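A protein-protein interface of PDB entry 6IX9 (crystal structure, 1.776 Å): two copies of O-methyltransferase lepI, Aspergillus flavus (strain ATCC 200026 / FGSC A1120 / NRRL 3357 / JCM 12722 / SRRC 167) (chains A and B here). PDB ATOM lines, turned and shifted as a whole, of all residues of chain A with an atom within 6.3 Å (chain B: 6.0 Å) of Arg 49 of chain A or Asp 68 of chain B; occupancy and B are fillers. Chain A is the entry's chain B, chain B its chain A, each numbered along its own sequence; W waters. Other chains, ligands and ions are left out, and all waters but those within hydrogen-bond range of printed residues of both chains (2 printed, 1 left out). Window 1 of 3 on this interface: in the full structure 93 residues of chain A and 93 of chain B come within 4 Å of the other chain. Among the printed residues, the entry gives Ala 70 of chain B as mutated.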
ATOM      1  N   ILE A  44      30.172   3.638  20.807  1.00  0.00           N
ATOM      2  CA  ILE A  44      29.173   3.304  19.786  1.00  0.00           C
ATOM      3  C   ILE A  44      28.063   2.460  20.398  1.00  0.00           C
ATOM      4  O   ILE A  44      26.869   2.705  20.157  1.00  0.00           O
ATOM      5  CB  ILE A  44      29.823   2.580  18.590  1.00  0.00           C
ATOM      6  CG1 ILE A  44      30.701   3.537  17.766  1.00  0.00           C
ATOM      7  CG2 ILE A  44      28.752   1.952  17.678  1.00  0.00           C
ATOM      8  CD1 ILE A  44      31.561   2.837  16.724  1.00  0.00           C
ATOM      9  N   ASN A  45      28.427   1.472  21.228  1.00  0.00           N
ATOM     10  CA  ASN A  45      27.360   0.624  21.760  1.00  0.00           C
ATOM     11  C   ASN A  45      26.458   1.388  22.718  1.00  0.00           C
ATOM     12  O   ASN A  45      25.245   1.169  22.728  1.00  0.00           O
ATOM     13  CB  ASN A  45      27.923  -0.624  22.429  1.00  0.00           C
ATOM     14  CG  ASN A  45      27.695  -1.835  21.574  1.00  0.00           C
ATOM     15  OD1 ASN A  45      27.778  -1.731  20.340  1.00  0.00           O
ATOM     16  ND2 ASN A  45      27.345  -2.965  22.184  1.00  0.00           N
ATOM     17  N   ASP A  46      26.994   2.339  23.484  1.00  0.00           N
ATOM     18  CA  ASP A  46      26.175   3.216  24.324  1.00  0.00           C
ATOM     19  C   ASP A  46      25.201   4.035  23.480  1.00  0.00           C
ATOM     20  O   ASP A  46      24.051   4.259  23.885  1.00  0.00           O
ATOM     21  CB  ASP A  46      27.060   4.154  25.143  1.00  0.00           C
ATOM     22  CG  ASP A  46      27.511   3.536  26.477  1.00  0.00           C
ATOM     23  OD1 ASP A  46      27.087   2.391  26.758  1.00  0.00           O
ATOM     24  OD2 ASP A  46      28.280   4.176  27.247  1.00  0.00           O
ATOM     25  N   ALA A  47      25.702   4.560  22.357  1.00  0.00           N
ATOM     26  CA  ALA A  47      24.852   5.332  21.447  1.00  0.00           C
ATOM     27  C   ALA A  47      23.752   4.469  20.836  1.00  0.00           C
ATOM     28  O   ALA A  47      22.618   4.937  20.641  1.00  0.00           O
ATOM     29  CB  ALA A  47      25.709   5.955  20.339  1.00  0.00           C
ATOM     30  N   LEU A  48      24.067   3.220  20.483  1.00  0.00           N
ATOM     31  CA  LEU A  48      23.039   2.338  19.936  1.00  0.00           C
ATOM     32  C   LEU A  48      21.937   2.082  20.961  1.00  0.00           C
ATOM     33  O   LEU A  48      20.746   2.061  20.620  1.00  0.00           O
ATOM     34  CB  LEU A  48      23.668   1.012  19.481  1.00  0.00           C
ATOM     35  CG  LEU A  48      24.668   1.022  18.322  1.00  0.00           C
ATOM     36  CD1 LEU A  48      25.248  -0.348  18.092  1.00  0.00           C
ATOM     37  CD2 LEU A  48      23.962   1.504  17.072  1.00  0.00           C
ATOM     38  N   ARG A  49      22.308   1.906  22.225  1.00  0.00           N
ATOM     39  CA  ARG A  49      21.294   1.732  23.259  1.00  0.00           C
ATOM     40  C   ARG A  49      20.439   2.988  23.422  1.00  0.00           C
ATOM     41  O   ARG A  49      19.203   2.896  23.512  1.00  0.00           O
ATOM     42  CB  ARG A  49      21.963   1.354  24.580  1.00  0.00           C
ATOM     43  CG  ARG A  49      20.996   1.169  25.692  1.00  0.00           C
ATOM     44  CD  ARG A  49      21.790   0.999  26.968  1.00  0.00           C
ATOM     45  NE  ARG A  49      22.326  -0.341  27.128  1.00  0.00           N
ATOM     46  CZ  ARG A  49      21.979  -1.131  28.150  1.00  0.00           C
ATOM     47  NH1 ARG A  49      22.509  -2.335  28.286  1.00  0.00           N
ATOM     48  NH2 ARG A  49      21.102  -0.686  29.046  1.00  0.00           N
ATOM     49  N   GLU A  50      21.061   4.171  23.470  1.00  0.00           N
ATOM     50  CA  GLU A  50      20.272   5.394  23.609  1.00  0.00           C
ATOM     51  C   GLU A  50      19.358   5.593  22.409  1.00  0.00           C
ATOM     52  O   GLU A  50      18.211   6.032  22.563  1.00  0.00           O
ATOM     53  CB  GLU A  50      21.174   6.616  23.802  1.00  0.00           C
ATOM     54  CG  GLU A  50      20.429   7.972  23.913  1.00  0.00           C
ATOM     55  CD  GLU A  50      19.351   8.023  25.013  1.00  0.00           C
ATOM     56  OE1 GLU A  50      19.565   8.675  26.060  1.00  0.00           O
ATOM     57  OE2 GLU A  50      18.269   7.439  24.827  1.00  0.00           O
ATOM     58  N   LEU A  51      19.837   5.266  21.206  1.00  0.00           N
ATOM     59  CA  LEU A  51      18.971   5.387  20.027  1.00  0.00           C
ATOM     60  C   LEU A  51      17.783   4.443  20.134  1.00  0.00           C
ATOM     61  O   LEU A  51      16.638   4.835  19.871  1.00  0.00           O
ATOM     62  CB  LEU A  51      19.754   5.085  18.755  1.00  0.00           C
ATOM     63  CG  LEU A  51      20.595   6.188  18.161  1.00  0.00           C
ATOM     64  CD1 LEU A  51      21.498   5.561  17.082  1.00  0.00           C
ATOM     65  CD2 LEU A  51      19.649   7.228  17.545  1.00  0.00           C
ATOM     66  N   GLN A  52      18.036   3.202  20.545  1.00  0.00           N
ATOM     67  CA  GLN A  52      16.957   2.235  20.715  1.00  0.00           C
ATOM     68  C   GLN A  52      15.878   2.758  21.670  1.00  0.00           C
ATOM     69  O   GLN A  52      14.676   2.657  21.386  1.00  0.00           O
ATOM     70  CB  GLN A  52      17.549   0.917  21.213  1.00  0.00           C
ATOM     71  CG  GLN A  52      16.561  -0.186  21.343  1.00  0.00           C
ATOM     72  CD  GLN A  52      17.170  -1.412  21.961  1.00  0.00           C
ATOM     73  OE1 GLN A  52      18.329  -1.750  21.690  1.00  0.00           O
ATOM     74  NE2 GLN A  52      16.395  -2.095  22.813  1.00  0.00           N
ATOM     75  N   TYR A  53      16.289   3.327  22.809  1.00  0.00           N
ATOM     76  CA  TYR A  53      15.324   3.812  23.790  1.00  0.00           C
ATOM     77  C   TYR A  53      14.562   5.032  23.275  1.00  0.00           C
ATOM     78  O   TYR A  53      13.362   5.178  23.535  1.00  0.00           O
ATOM     79  CB  TYR A  53      16.034   4.158  25.103  1.00  0.00           C
ATOM     80  CG  TYR A  53      16.639   2.998  25.854  1.00  0.00           C
ATOM     81  CD1 TYR A  53      16.277   1.688  25.589  1.00  0.00           C
ATOM     82  CD2 TYR A  53      17.600   3.225  26.845  1.00  0.00           C
ATOM     83  CE1 TYR A  53      16.857   0.615  26.320  1.00  0.00           C
ATOM     84  CE2 TYR A  53      18.169   2.182  27.570  1.00  0.00           C
ATOM     85  CZ  TYR A  53      17.784   0.879  27.313  1.00  0.00           C
ATOM     86  OH  TYR A  53      18.368  -0.154  28.035  1.00  0.00           O
ATOM     87  N   SER A  54      15.238   5.920  22.544  1.00  0.00           N
ATOM     88  CA  SER A  54      14.546   7.094  22.026  1.00  0.00           C
ATOM     89  C   SER A  54      13.568   6.748  20.903  1.00  0.00           C
ATOM     90  O   SER A  54      12.582   7.474  20.715  1.00  0.00           O
ATOM     91  CB  SER A  54      15.557   8.130  21.539  1.00  0.00           C
ATOM     92  OG  SER A  54      16.206   7.657  20.380  1.00  0.00           O
ATOM     93  N   ASP A  68      13.126  -8.562  28.707  1.00  0.00           N
ATOM     94  CA  ASP A  68      14.589  -8.630  28.697  1.00  0.00           C
ATOM     95  C   ASP A  68      15.123  -9.422  29.889  1.00  0.00           C
ATOM     96  O   ASP A  68      16.181 -10.059  29.790  1.00  0.00           O
ATOM     97  CB  ASP A  68      15.194  -7.218  28.656  1.00  0.00           C
ATOM     98  CG  ASP A  68      15.269  -6.639  27.221  1.00  0.00           C
ATOM     99  OD1 ASP A  68      14.749  -7.266  26.246  1.00  0.00           O
ATOM    100  OD2 ASP A  68      15.855  -5.544  27.065  1.00  0.00           O
ATOM    101  N   THR A  69      14.398  -9.436  31.012  1.00  0.00           N
ATOM    102  CA  THR A  69      14.867 -10.237  32.146  1.00  0.00           C
ATOM    103  C   THR A  69      14.802 -11.752  31.883  1.00  0.00           C
ATOM    104  O   THR A  69      15.550 -12.507  32.512  1.00  0.00           O
ATOM    105  CB  THR A  69      14.080  -9.860  33.398  1.00  0.00           C
ATOM    106  OG1 THR A  69      12.673  -9.834  33.098  1.00  0.00           O
ATOM    107  CG2 THR A  69      14.519  -8.474  33.865  1.00  0.00           C
ATOM    108  N   TRP A 351      25.082   3.773  32.128  1.00  0.00           N
ATOM    109  CA  TRP A 351      24.277   2.738  32.784  1.00  0.00           C
ATOM    110  C   TRP A 351      25.130   1.711  33.517  1.00  0.00           C
ATOM    111  O   TRP A 351      24.705   1.194  34.555  1.00  0.00           O
ATOM    112  CB  TRP A 351      23.352   2.026  31.779  1.00  0.00           C
ATOM    113  CG  TRP A 351      24.092   1.237  30.718  1.00  0.00           C
ATOM    114  CD1 TRP A 351      24.514   1.694  29.498  1.00  0.00           C
ATOM    115  CD2 TRP A 351      24.512  -0.129  30.808  1.00  0.00           C
ATOM    116  NE1 TRP A 351      25.180   0.683  28.820  1.00  0.00           N
ATOM    117  CE2 TRP A 351      25.190  -0.442  29.611  1.00  0.00           C
ATOM    118  CE3 TRP A 351      24.384  -1.122  31.795  1.00  0.00           C
ATOM    119  CZ2 TRP A 351      25.743  -1.711  29.364  1.00  0.00           C
ATOM    120  CZ3 TRP A 351      24.939  -2.376  31.555  1.00  0.00           C
ATOM    121  CH2 TRP A 351      25.592  -2.668  30.338  1.00  0.00           C
ATOM    122  N   GLN B  52      24.176  -4.081  18.856  1.00  0.00           N
ATOM    123  CA  GLN B  52      24.659  -4.012  20.232  1.00  0.00           C
ATOM    124  C   GLN B  52      25.157  -5.373  20.721  1.00  0.00           C
ATOM    125  O   GLN B  52      26.246  -5.475  21.296  1.00  0.00           O
ATOM    126  CB  GLN B  52      23.543  -3.490  21.136  1.00  0.00           C
ATOM    127  CG  GLN B  52      23.914  -3.413  22.580  1.00  0.00           C
ATOM    128  CD  GLN B  52      22.755  -2.947  23.433  1.00  0.00           C
ATOM    129  OE1 GLN B  52      21.936  -2.143  22.993  1.00  0.00           O
ATOM    130  NE2 GLN B  52      22.677  -3.451  24.666  1.00  0.00           N
ATOM    131  N   MET B  63      27.711  -7.841  32.095  1.00  0.00           N
ATOM    132  CA  MET B  63      27.245  -6.631  32.768  1.00  0.00           C
ATOM    133  C   MET B  63      25.811  -6.312  32.376  1.00  0.00           C
ATOM    134  O   MET B  63      24.976  -5.979  33.225  1.00  0.00           O
ATOM    135  CB  MET B  63      28.156  -5.456  32.424  1.00  0.00           C
ATOM    136  CG  MET B  63      28.040  -4.297  33.377  1.00  0.00           C
ATOM    137  SD  MET B  63      28.711  -4.750  34.988  1.00  0.00           S
ATOM    138  CE  MET B  63      29.874  -3.415  35.231  1.00  0.00           C
ATOM    139  N   ARG B  64      25.511  -6.403  31.079  1.00  0.00           N
ATOM    140  CA  ARG B  64      24.152  -6.147  30.613  1.00  0.00           C
ATOM    141  C   ARG B  64      23.171  -7.132  31.244  1.00  0.00           C
ATOM    142  O   ARG B  64      22.103  -6.741  31.744  1.00  0.00           O
ATOM    143  CB  ARG B  64      24.148  -6.226  29.080  1.00  0.00           C
ATOM    144  CG  ARG B  64      22.884  -6.551  28.466  1.00  0.00           C
ATOM    145  CD  ARG B  64      22.983  -6.452  26.964  1.00  0.00           C
ATOM    146  NE  ARG B  64      23.501  -7.650  26.296  1.00  0.00           N
ATOM    147  CZ  ARG B  64      22.851  -8.806  26.159  1.00  0.00           C
ATOM    148  NH1 ARG B  64      21.640  -9.001  26.696  1.00  0.00           N
ATOM    149  NH2 ARG B  64      23.431  -9.783  25.485  1.00  0.00           N
ATOM    150  N   MET B  65      23.520  -8.425  31.247  1.00  0.00           N
ATOM    151  CA  MET B  65      22.653  -9.399  31.903  1.00  0.00           C
ATOM    152  C   MET B  65      22.544  -9.150  33.411  1.00  0.00           C
ATOM    153  O   MET B  65      21.482  -9.398  34.010  1.00  0.00           O
ATOM    154  CB  MET B  65      23.151 -10.816  31.597  1.00  0.00           C
ATOM    155  CG  MET B  65      22.850 -11.229  30.174  1.00  0.00           C
ATOM    156  SD  MET B  65      23.347 -12.943  29.888  1.00  0.00           S
ATOM    157  CE  MET B  65      23.004 -13.013  28.126  1.00  0.00           C
ATOM    158  N   SER B  66      23.589  -8.607  34.039  1.00  0.00           N
ATOM    159  CA  SER B  66      23.507  -8.350  35.477  1.00  0.00           C
ATOM    160  C   SER B  66      22.623  -7.146  35.784  1.00  0.00           C
ATOM    161  O   SER B  66      21.925  -7.128  36.803  1.00  0.00           O
ATOM    162  CB  SER B  66      24.905  -8.108  36.068  1.00  0.00           C
ATOM    163  OG  SER B  66      25.746  -9.234  35.950  1.00  0.00           O
ATOM    164  N   LEU B  67      22.641  -6.125  34.926  1.00  0.00           N
ATOM    165  CA  LEU B  67      22.085  -4.825  35.297  1.00  0.00           C
ATOM    166  C   LEU B  67      20.763  -4.486  34.626  1.00  0.00           C
ATOM    167  O   LEU B  67      19.989  -3.713  35.201  1.00  0.00           O
ATOM    168  CB  LEU B  67      23.084  -3.691  34.983  1.00  0.00           C
ATOM    169  CG  LEU B  67      24.404  -3.738  35.754  1.00  0.00           C
ATOM    170  CD1 LEU B  67      25.340  -2.554  35.410  1.00  0.00           C
ATOM    171  CD2 LEU B  67      24.170  -3.837  37.286  1.00  0.00           C
ATOM    172  N   ASP B  68      20.465  -5.033  33.442  1.00  0.00           N
ATOM    173  CA  ASP B  68      19.240  -4.603  32.764  1.00  0.00           C
ATOM    174  C   ASP B  68      17.989  -4.988  33.558  1.00  0.00           C
ATOM    175  O   ASP B  68      16.951  -4.326  33.436  1.00  0.00           O
ATOM    176  CB  ASP B  68      19.186  -5.162  31.336  1.00  0.00           C
ATOM    177  CG  ASP B  68      20.119  -4.400  30.335  1.00  0.00           C
ATOM    178  OD1 ASP B  68      20.836  -3.420  30.698  1.00  0.00           O
ATOM    179  OD2 ASP B  68      20.122  -4.785  29.146  1.00  0.00           O
ATOM    180  N   THR B  69      18.092  -6.001  34.419  1.00  0.00           N
ATOM    181  CA  THR B  69      17.034  -6.348  35.374  1.00  0.00           C
ATOM    182  C   THR B  69      16.622  -5.171  36.266  1.00  0.00           C
ATOM    183  O   THR B  69      15.457  -5.052  36.681  1.00  0.00           O
ATOM    184  CB  THR B  69      17.550  -7.471  36.268  1.00  0.00           C
ATOM    185  OG1 THR B  69      18.218  -8.462  35.475  1.00  0.00           O
ATOM    186  CG2 THR B  69      16.438  -8.085  36.974  1.00  0.00           C
ATOM    187  N   ALA B  70      17.578  -4.333  36.637  1.00  0.00           N
ATOM    188  CA  ALA B  70      17.315  -3.247  37.568  1.00  0.00           C
ATOM    189  C   ALA B  70      16.346  -2.225  37.001  1.00  0.00           C
ATOM    190  O   ALA B  70      15.745  -1.474  37.764  1.00  0.00           O
ATOM    191  CB  ALA B  70      18.633  -2.567  37.942  1.00  0.00           C
ATOM    192  N   GLN B  71      16.205  -2.149  35.675  1.00  0.00           N
ATOM    193  CA  GLN B  71      15.281  -1.166  35.102  1.00  0.00           C
ATOM    194  C   GLN B  71      13.870  -1.394  35.600  1.00  0.00           C
ATOM    195  O   GLN B  71      13.159  -0.432  35.931  1.00  0.00           O
ATOM    196  CB  GLN B  71      15.287  -1.222  33.577  1.00  0.00           C
ATOM    197  CG  GLN B  71      16.617  -0.822  32.981  1.00  0.00           C
ATOM    198  CD  GLN B  71      16.510  -0.427  31.532  1.00  0.00           C
ATOM    199  OE1 GLN B  71      15.486   0.098  31.079  1.00  0.00           O
ATOM    200  NE2 GLN B  71      17.593  -0.654  30.791  1.00  0.00           N
ATOM    201  N   VAL B  72      13.437  -2.658  35.640  1.00  0.00           N
ATOM    202  CA  VAL B  72      12.069  -2.951  36.054  1.00  0.00           C
ATOM    203  C   VAL B  72      11.871  -2.621  37.531  1.00  0.00           C
ATOM    204  O   VAL B  72      10.829  -2.097  37.917  1.00  0.00           O
ATOM    205  CB  VAL B  72      11.696  -4.416  35.765  1.00  0.00           C
ATOM    206  CG1 VAL B  72      10.231  -4.596  36.077  1.00  0.00           C
ATOM    207  CG2 VAL B  72      11.993  -4.797  34.303  1.00  0.00           C
ATOM    208  N   TYR B 116      20.545   6.890  37.839  1.00  0.00           N
ATOM    209  CA  TYR B 116      20.324   5.642  37.142  1.00  0.00           C
ATOM    210  C   TYR B 116      19.244   5.794  36.076  1.00  0.00           C
ATOM    211  O   TYR B 116      19.427   5.357  34.937  1.00  0.00           O
ATOM    212  CB  TYR B 116      19.940   4.566  38.140  1.00  0.00           C
ATOM    213  CG  TYR B 116      19.553   3.319  37.428  1.00  0.00           C
ATOM    214  CD1 TYR B 116      20.510   2.543  36.806  1.00  0.00           C
ATOM    215  CD2 TYR B 116      18.220   2.955  37.303  1.00  0.00           C
ATOM    216  CE1 TYR B 116      20.154   1.391  36.123  1.00  0.00           C
ATOM    217  CE2 TYR B 116      17.864   1.825  36.618  1.00  0.00           C
ATOM    218  CZ  TYR B 116      18.842   1.044  36.046  1.00  0.00           C
ATOM    219  OH  TYR B 116      18.503  -0.084  35.368  1.00  0.00           O
ATOM    220  N   SER B 119      20.422   7.452  32.956  1.00  0.00           N
ATOM    221  CA  SER B 119      21.365   6.664  32.166  1.00  0.00           C
ATOM    222  C   SER B 119      20.667   5.617  31.298  1.00  0.00           C
ATOM    223  O   SER B 119      21.295   5.067  30.382  1.00  0.00           O
ATOM    224  CB  SER B 119      22.391   5.998  33.098  1.00  0.00           C
ATOM    225  OG  SER B 119      21.834   4.876  33.745  1.00  0.00           O
ATOM    226  N   VAL B 120      19.391   5.322  31.554  1.00  0.00           N
ATOM    227  CA  VAL B 120      18.615   4.408  30.711  1.00  0.00           C
ATOM    228  C   VAL B 120      17.398   5.121  30.114  1.00  0.00           C
ATOM    229  O   VAL B 120      16.439   4.476  29.677  1.00  0.00           O
ATOM    230  CB  VAL B 120      18.220   3.125  31.481  1.00  0.00           C
ATOM    231  CG1 VAL B 120      19.470   2.276  31.812  1.00  0.00           C
ATOM    232  CG2 VAL B 120      17.491   3.457  32.780  1.00  0.00           C
HETATM  233  O   HOH W   1      24.185   5.135  29.816  1.00  0.00           O
HETATM  234  O   HOH W   2      20.465  -3.906  26.742  1.00  0.00           O
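The side-chain amide nitrogen of Asn 45 of chain A lies within hydrogen-bond range of the backbone carbonyl oxygen of Gln 52 of chain B, at 2.9 Å. NH1 of Arg 49 of chain A lies within salt-bridge range of OD1 of Asp 68 of chain B, 3.1 Å away. The side-chain amide nitrogen of Gln 71 of chain B sits at hydrogen-bond distance from the side-chain hydroxyl of Tyr 53 of chain A.
Gln 52 of chain A touches its own counterpart, Gln 52 of chain B. Thr 69 of chain A touches its own counterpart, Thr 69 of chain B.
OH of Tyr 116 of chain B sits at hydrogen-bond distance from N of Gln 71 of chain B (3.1 Å). The backbone carbonyl oxygen of Tyr 116 of chain B sits at hydrogen-bond distance from the side-chain hydroxyl of Ser 119 of chain B (2.7 Å). OD1 of Asp 46 of chain A lies within hydrogen-bond range of NE1 of Trp 351 of chain A, at 3.3 Å. OH of Tyr 53 of chain A is in hydrogen-bond range of NH2 of Arg 49 of chain A, at 3.0 Å.
Of the 14 printed residues of chain B, 9 touch a printed residue of chain A. Hydrophobic or aromatic side chains of chain B within 4 Å of the printed part of chain A: Leu 67 and Val 120. Hydrophobic or aromatic side chains of chain A that line the printed part of chain B: Leu 48, Tyr 53 and Trp 351. Among the printed residues, 14 pairs touch across the chains.
Of chain A, only Arg 49 (3.1 Å) comes within 4 Å of Asp 68 of chain B. Of the printed residues of chain B, Tyr 53 of chain A touches Gln 71 and Val 120. Printed residues of chain A within 4 Å of Arg 64 of chain B: Trp 351 (3.8 Å). Printed residues of chain A within 4 Å of Val 120 of chain B: Tyr 53 and Trp 351. Ser 66 of chain B touches none of the printed residues of chain A. Asp 46 of chain A touches none of the printed residues of chain B. The nearest printed residue of chain B that does not touch Arg 49 of chain A is Arg 64 of chain B (4.2 Å).
Gln 52 of chain B touches Leu 48 of chain A. Gln 52 of chain B touches Arg 49 of chain A (NE2 to NH1, 3.8 Å). Gln 71 of chain B touches Arg 49 of chain A (NE2 to NH2, 3.9 Å). OE1 of Gln 52 of chain A touches OE1 of Gln 52 of chain B, 3.9 Å away. CD2 of Tyr 53 of chain A touches O of Val 120 of chain B, at 3.3 Å. CA of Thr 69 of chain B touches CG2 of Thr 69 of chain A (3.6 Å). CZ3 of Trp 351 of chain A touches O of Met 63 of chain B (3.97 Å). Trp 351 of chain A touches Arg 64 of chain B (CH2 to CA, 3.8 Å). Trp 351 of chain A touches Leu 67 of chain B. CG1 of Val 120 of chain B touches CB of Trp 351 of chain A (3.9 Å).
Water W2 lies within hydrogen-bond range of the side-chain carboxylate (OD2) of Asp 68 of chain B, the guanidinium group (NH1) of Arg 49 of chain A and the side-chain amide nitrogen (NE2) of Gln 52 of chain B. Water W1 lies within hydrogen-bond range of N of Trp 351 of chain A (2.8 Å) and O of Ser 119 of chain B (2.9 Å).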
